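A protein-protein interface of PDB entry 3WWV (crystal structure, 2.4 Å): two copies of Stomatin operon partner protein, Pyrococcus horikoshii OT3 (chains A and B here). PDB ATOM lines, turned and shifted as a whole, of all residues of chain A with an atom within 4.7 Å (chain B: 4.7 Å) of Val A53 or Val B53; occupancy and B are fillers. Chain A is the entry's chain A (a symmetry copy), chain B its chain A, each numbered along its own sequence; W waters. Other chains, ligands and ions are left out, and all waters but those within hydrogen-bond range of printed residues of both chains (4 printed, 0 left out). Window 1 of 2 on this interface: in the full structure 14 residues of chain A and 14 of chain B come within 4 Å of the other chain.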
ATOM      1  N   ILE A  11     -11.148   6.634   4.867  1.00  0.00           N
ATOM      2  CA  ILE A  11     -11.055   7.377   3.626  1.00  0.00           C
ATOM      3  C   ILE A  11     -12.348   7.262   2.805  1.00  0.00           C
ATOM      4  O   ILE A  11     -12.888   6.172   2.604  1.00  0.00           O
ATOM      5  CB  ILE A  11      -9.771   6.998   2.838  1.00  0.00           C
ATOM      6  CG1 ILE A  11      -8.545   7.505   3.602  1.00  0.00           C
ATOM      7  CG2 ILE A  11      -9.783   7.607   1.441  1.00  0.00           C
ATOM      8  CD1 ILE A  11      -7.212   7.088   3.019  1.00  0.00           C
ATOM      9  N   LYS A  39      -6.843  19.705   3.611  1.00  0.00           N
ATOM     10  CA  LYS A  39      -5.721  19.466   2.702  1.00  0.00           C
ATOM     11  C   LYS A  39      -5.174  20.728   2.029  1.00  0.00           C
ATOM     12  O   LYS A  39      -3.963  20.892   1.949  1.00  0.00           O
ATOM     13  CB  LYS A  39      -6.063  18.426   1.644  1.00  0.00           C
ATOM     14  CG  LYS A  39      -4.821  17.911   0.925  1.00  0.00           C
ATOM     15  CD  LYS A  39      -5.145  16.828  -0.078  1.00  0.00           C
ATOM     16  CE  LYS A  39      -3.944  16.585  -0.970  1.00  0.00           C
ATOM     17  NZ  LYS A  39      -2.905  15.757  -0.305  1.00  0.00           N
ATOM     18  N   ARG A  51     -15.104  15.770   3.394  1.00  0.00           N
ATOM     19  CA  ARG A  51     -14.848  14.435   2.877  1.00  0.00           C
ATOM     20  C   ARG A  51     -13.465  13.982   3.343  1.00  0.00           C
ATOM     21  O   ARG A  51     -12.516  14.744   3.239  1.00  0.00           O
ATOM     22  CB  ARG A  51     -14.859  14.493   1.350  1.00  0.00           C
ATOM     23  CG  ARG A  51     -14.919  13.141   0.651  1.00  0.00           C
ATOM     24  CD  ARG A  51     -16.303  12.900   0.079  1.00  0.00           C
ATOM     25  NE  ARG A  51     -17.023  11.892   0.831  1.00  0.00           N
ATOM     26  CZ  ARG A  51     -18.322  11.642   0.710  1.00  0.00           C
ATOM     27  NH1 ARG A  51     -19.075  12.350  -0.120  1.00  0.00           N
ATOM     28  NH2 ARG A  51     -18.874  10.686   1.438  1.00  0.00           N
ATOM     29  N   VAL A  52     -13.342  12.750   3.831  1.00  0.00           N
ATOM     30  CA  VAL A  52     -12.039  12.239   4.275  1.00  0.00           C
ATOM     31  C   VAL A  52     -11.242  11.699   3.076  1.00  0.00           C
ATOM     32  O   VAL A  52     -11.699  10.780   2.405  1.00  0.00           O
ATOM     33  CB  VAL A  52     -12.176  11.147   5.372  1.00  0.00           C
ATOM     34  CG1 VAL A  52     -10.812  10.793   5.954  1.00  0.00           C
ATOM     35  CG2 VAL A  52     -13.124  11.592   6.483  1.00  0.00           C
ATOM     36  N   VAL A  53     -10.064  12.268   2.810  1.00  0.00           N
ATOM     37  CA  VAL A  53      -9.288  11.909   1.611  1.00  0.00           C
ATOM     38  C   VAL A  53      -7.983  11.168   1.907  1.00  0.00           C
ATOM     39  O   VAL A  53      -7.425  10.500   1.022  1.00  0.00           O
ATOM     40  CB  VAL A  53      -9.010  13.124   0.682  1.00  0.00           C
ATOM     41  CG1 VAL A  53     -10.320  13.715   0.165  1.00  0.00           C
ATOM     42  CG2 VAL A  53      -8.178  14.195   1.383  1.00  0.00           C
ATOM     43  N   ASP A  54      -7.499  11.286   3.143  1.00  0.00           N
ATOM     44  CA  ASP A  54      -6.256  10.632   3.575  1.00  0.00           C
ATOM     45  C   ASP A  54      -6.186  10.615   5.091  1.00  0.00           C
ATOM     46  O   ASP A  54      -7.071  11.138   5.763  1.00  0.00           O
ATOM     47  CB  ASP A  54      -5.036  11.374   3.015  1.00  0.00           C
ATOM     48  CG  ASP A  54      -3.795  10.504   2.935  1.00  0.00           C
ATOM     49  OD1 ASP A  54      -3.840   9.291   3.255  1.00  0.00           O
ATOM     50  OD2 ASP A  54      -2.749  11.050   2.541  1.00  0.00           O
ATOM     51  N   ILE A  61      -7.272  13.812   7.061  1.00  0.00           N
ATOM     52  CA  ILE A  61      -7.065  14.871   6.069  1.00  0.00           C
ATOM     53  C   ILE A  61      -8.316  14.944   5.223  1.00  0.00           C
ATOM     54  O   ILE A  61      -8.812  13.930   4.733  1.00  0.00           O
ATOM     55  CB  ILE A  61      -5.788  14.633   5.245  1.00  0.00           C
ATOM     56  CG1 ILE A  61      -4.578  14.709   6.186  1.00  0.00           C
ATOM     57  CG2 ILE A  61      -5.629  15.667   4.128  1.00  0.00           C
ATOM     58  CD1 ILE A  61      -3.424  13.849   5.741  1.00  0.00           C
ATOM     59  N   VAL A  62      -8.855  16.151   5.095  1.00  0.00           N
ATOM     60  CA  VAL A  62     -10.199  16.352   4.575  1.00  0.00           C
ATOM     61  C   VAL A  62     -10.185  17.506   3.589  1.00  0.00           C
ATOM     62  O   VAL A  62      -9.313  18.384   3.666  1.00  0.00           O
ATOM     63  CB  VAL A  62     -11.214  16.656   5.706  1.00  0.00           C
ATOM     64  CG1 VAL A  62     -11.248  15.544   6.748  1.00  0.00           C
ATOM     65  CG2 VAL A  62     -10.912  17.979   6.387  1.00  0.00           C
ATOM     66  N   VAL A  63     -11.128  17.476   2.651  1.00  0.00           N
ATOM     67  CA  VAL A  63     -11.493  18.639   1.833  1.00  0.00           C
ATOM     68  C   VAL A  63     -12.953  18.943   2.159  1.00  0.00           C
ATOM     69  O   VAL A  63     -13.666  18.057   2.642  1.00  0.00           O
ATOM     70  CB  VAL A  63     -11.325  18.385   0.303  1.00  0.00           C
ATOM     71  CG1 VAL A  63      -9.857  18.145  -0.050  1.00  0.00           C
ATOM     72  CG2 VAL A  63     -12.186  17.223  -0.182  1.00  0.00           C
ATOM     73  N   ILE B  11      -9.626  16.625  -6.376  1.00  0.00           N
ATOM     74  CA  ILE B  11      -9.828  15.888  -5.144  1.00  0.00           C
ATOM     75  C   ILE B  11     -11.225  16.148  -4.559  1.00  0.00           C
ATOM     76  O   ILE B  11     -11.672  17.291  -4.444  1.00  0.00           O
ATOM     77  CB  ILE B  11      -8.668  16.135  -4.142  1.00  0.00           C
ATOM     78  CG1 ILE B  11      -7.388  15.493  -4.687  1.00  0.00           C
ATOM     79  CG2 ILE B  11      -8.986  15.544  -2.774  1.00  0.00           C
ATOM     80  CD1 ILE B  11      -6.140  15.772  -3.878  1.00  0.00           C
ATOM     81  N   LYS B  39      -7.023   3.182  -4.515  1.00  0.00           N
ATOM     82  CA  LYS B  39      -6.056   3.308  -3.423  1.00  0.00           C
ATOM     83  C   LYS B  39      -5.772   2.002  -2.677  1.00  0.00           C
ATOM     84  O   LYS B  39      -4.617   1.710  -2.390  1.00  0.00           O
ATOM     85  CB  LYS B  39      -6.463   4.389  -2.431  1.00  0.00           C
ATOM     86  CG  LYS B  39      -5.317   4.775  -1.502  1.00  0.00           C
ATOM     87  CD  LYS B  39      -5.692   5.895  -0.561  1.00  0.00           C
ATOM     88  CE  LYS B  39      -4.645   6.017   0.528  1.00  0.00           C
ATOM     89  NZ  LYS B  39      -3.424   6.724   0.061  1.00  0.00           N
ATOM     90  N   ARG B  51     -14.729   7.977  -5.695  1.00  0.00           N
ATOM     91  CA  ARG B  51     -14.425   9.284  -5.129  1.00  0.00           C
ATOM     92  C   ARG B  51     -12.942   9.582  -5.345  1.00  0.00           C
ATOM     93  O   ARG B  51     -12.112   8.723  -5.085  1.00  0.00           O
ATOM     94  CB  ARG B  51     -14.707   9.240  -3.628  1.00  0.00           C
ATOM     95  CG  ARG B  51     -14.743  10.597  -2.937  1.00  0.00           C
ATOM     96  CD  ARG B  51     -16.171  10.990  -2.611  1.00  0.00           C
ATOM     97  NE  ARG B  51     -16.637  12.062  -3.467  1.00  0.00           N
ATOM     98  CZ  ARG B  51     -17.904  12.451  -3.571  1.00  0.00           C
ATOM     99  NH1 ARG B  51     -18.860  11.834  -2.890  1.00  0.00           N
ATOM    100  NH2 ARG B  51     -18.217  13.453  -4.375  1.00  0.00           N
ATOM    101  N   VAL B  52     -12.605  10.788  -5.792  1.00  0.00           N
ATOM    102  CA  VAL B  52     -11.199  11.153  -5.999  1.00  0.00           C
ATOM    103  C   VAL B  52     -10.568  11.616  -4.675  1.00  0.00           C
ATOM    104  O   VAL B  52     -11.034  12.586  -4.085  1.00  0.00           O
ATOM    105  CB  VAL B  52     -11.026  12.243  -7.093  1.00  0.00           C
ATOM    106  CG1 VAL B  52      -9.553  12.445  -7.426  1.00  0.00           C
ATOM    107  CG2 VAL B  52     -11.810  11.892  -8.356  1.00  0.00           C
ATOM    108  N   VAL B  53      -9.522  10.928  -4.215  1.00  0.00           N
ATOM    109  CA  VAL B  53      -8.930  11.212  -2.896  1.00  0.00           C
ATOM    110  C   VAL B  53      -7.523  11.808  -2.955  1.00  0.00           C
ATOM    111  O   VAL B  53      -7.060  12.421  -1.980  1.00  0.00           O
ATOM    112  CB  VAL B  53      -8.950   9.983  -1.945  1.00  0.00           C
ATOM    113  CG1 VAL B  53     -10.384   9.541  -1.668  1.00  0.00           C
ATOM    114  CG2 VAL B  53      -8.127   8.823  -2.501  1.00  0.00           C
ATOM    115  N   ASP B  54      -6.848  11.627  -4.090  1.00  0.00           N
ATOM    116  CA  ASP B  54      -5.486  12.140  -4.293  1.00  0.00           C
ATOM    117  C   ASP B  54      -5.153  12.136  -5.774  1.00  0.00           C
ATOM    118  O   ASP B  54      -5.959  11.704  -6.594  1.00  0.00           O
ATOM    119  CB  ASP B  54      -4.468  11.278  -3.537  1.00  0.00           C
ATOM    120  CG  ASP B  54      -3.174  12.011  -3.235  1.00  0.00           C
ATOM    121  OD1 ASP B  54      -3.033  13.219  -3.548  1.00  0.00           O
ATOM    122  OD2 ASP B  54      -2.276  11.361  -2.672  1.00  0.00           O
ATOM    123  N   ILE B  61      -6.216   9.055  -7.932  1.00  0.00           N
ATOM    124  CA  ILE B  61      -6.299   7.989  -6.929  1.00  0.00           C
ATOM    125  C   ILE B  61      -7.678   8.058  -6.313  1.00  0.00           C
ATOM    126  O   ILE B  61      -8.140   9.124  -5.907  1.00  0.00           O
ATOM    127  CB  ILE B  61      -5.166   8.097  -5.894  1.00  0.00           C
ATOM    128  CG1 ILE B  61      -3.827   7.884  -6.612  1.00  0.00           C
ATOM    129  CG2 ILE B  61      -5.314   7.062  -4.776  1.00  0.00           C
ATOM    130  CD1 ILE B  61      -2.681   8.619  -5.966  1.00  0.00           C
ATOM    131  N   VAL B  62      -8.357   6.916  -6.292  1.00  0.00           N
ATOM    132  CA  VAL B  62      -9.784   6.865  -6.014  1.00  0.00           C
ATOM    133  C   VAL B  62     -10.064   5.725  -5.051  1.00  0.00           C
ATOM    134  O   VAL B  62      -9.291   4.759  -4.985  1.00  0.00           O
ATOM    135  CB  VAL B  62     -10.614   6.660  -7.307  1.00  0.00           C
ATOM    136  CG1 VAL B  62     -10.348   7.760  -8.328  1.00  0.00           C
ATOM    137  CG2 VAL B  62     -10.342   5.306  -7.938  1.00  0.00           C
ATOM    138  N   VAL B  63     -11.146   5.864  -4.291  1.00  0.00           N
ATOM    139  CA  VAL B  63     -11.769   4.755  -3.559  1.00  0.00           C
ATOM    140  C   VAL B  63     -13.175   4.604  -4.136  1.00  0.00           C
ATOM    141  O   VAL B  63     -13.695   5.558  -4.727  1.00  0.00           O
ATOM    142  CB  VAL B  63     -11.843   5.003  -2.021  1.00  0.00           C
ATOM    143  CG1 VAL B  63     -10.441   5.090  -1.417  1.00  0.00           C
ATOM    144  CG2 VAL B  63     -12.646   6.255  -1.682  1.00  0.00           C
HETATM  145  O   HOH W   1      -5.052   9.295  -0.187  1.00  0.00           O
HETATM  146  O   HOH W   2      -4.816  13.376  -0.367  1.00  0.00           O
HETATM  147  O   HOH W   3      -1.210  14.867  -1.829  1.00  0.00           O
HETATM  148  O   HOH W   4      -1.934   7.442   1.863  1.00  0.00           O
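Ile A11 touches Lys B39, and with the chains exchanged Lys A39 touches Ile B11. Ile A11 touches Val B53, and with the chains exchanged Val A53 touches Ile B11. Ile A11 touches Val B63, and with the chains exchanged Val A63 touches Ile B11. Arg B51 touches its own counterpart, Arg A51. 9 positions are printed for both chains. Of the 8 pairs that touch across the chains among the printed residues, 8 have their exchanged pair printed and touching as well.
The guanidinium group (NH1) of Arg A51 sits close to the guanidinium group (NH1) of Arg B51 (2.8 Å).
Printed residues of chain B within 4 Å of Arg A51: Arg B51 (2.8 Å). Val A53 touches just these residues of chain B: Ile B11 and Val B53. Asp A54 touches none of the printed residues of chain B. Printed residues of chain A within 4 Å of Lys B39: Ile A11. Of the printed residues of chain A, Arg B51 touches Arg A51. Of chain A, only Ile A11 and Val A53 come within 4 Å of Val B53. Asp B54 touches none of the printed residues of chain A. The nearest residue of chain B that does not touch Val A53 is Val B52 (4.5 Å). The nearest printed residue of chain B that does not touch Lys A39 is Asp B54 (4.1 Å).
Of the 9 printed residues of chain A, 5 touch a printed residue of chain B. Printed residues of chain A that touch a printed residue of chain B: Ile A11, Lys A39, Arg A51, Val A53 and Val A63. Hydrophobic or aromatic side chains of chain A within 4 Å of the printed part of chain B: Ile A11, Val A53 and Val A63. Hydrophobic or aromatic side chains of chain B that line the printed part of chain A: Ile B11, Val B53 and Val B63. Along chain B the printed residues that touch a printed residue of chain A span positions 11 to 63. Among the printed residues, 8 pairs touch across the chains. Among the printed residues, no Asp or Glu carboxylate lies within 4 Å of a Lys or Arg side-chain nitrogen of the other chain.
Water W3 lies within hydrogen-bond range of NZ of Lys A39 and OD1 of Asp B54. Water W4 bridges the side-chain amino group of Lys B39 and the side-chain carboxylate of Asp A54. Water W2 bridges the backbone carbonyl oxygen of Val B53 and the side-chain amino group of Lys A39. Water W1 bridges O of Val A53 and NZ of Lys B39.
CD1 of Ile A11 touches CE of Lys B39, 3.7 Å away. CG2 of Ile A11 touches CG1 of Val B53, 3.7 Å away. CG1 of Val B63 touches CG2 of Ile A11, 3.9 Å away. CD1 of Ile B11 touches CE of Lys A39, 3.7 Å away. Ile B11 touches Val A53 (CG2 to CG1, 3.7 Å). CB of Val A53 touches O of Val B53 (3.4 Å). Val A63 touches Ile B11 (CG1 to CG2, 3.9 Å).
O of Val B62 is in hydrogen-bond range of N of Lys B39 (2.8 Å). The backbone NH of Arg B51 lies within hydrogen-bond range of the backbone carbonyl oxygen of Val B63, at 2.8 Å. The backbone carbonyl oxygen (O) of Ile B61 lies within hydrogen-bond range of the backbone NH (N) of Val B53 (2.8 Å). The backbone NH of Lys A39 sits at hydrogen-bond distance from the backbone carbonyl oxygen of Val A62, 2.8 Å away. The backbone carbonyl oxygen (O) of Val A63 lies within hydrogen-bond range of the backbone NH (N) of Arg A51, at 2.8 Å. The backbone NH (N) of Val A53 sits at hydrogen-bond distance from the backbone carbonyl oxygen (O) of Ile A61.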
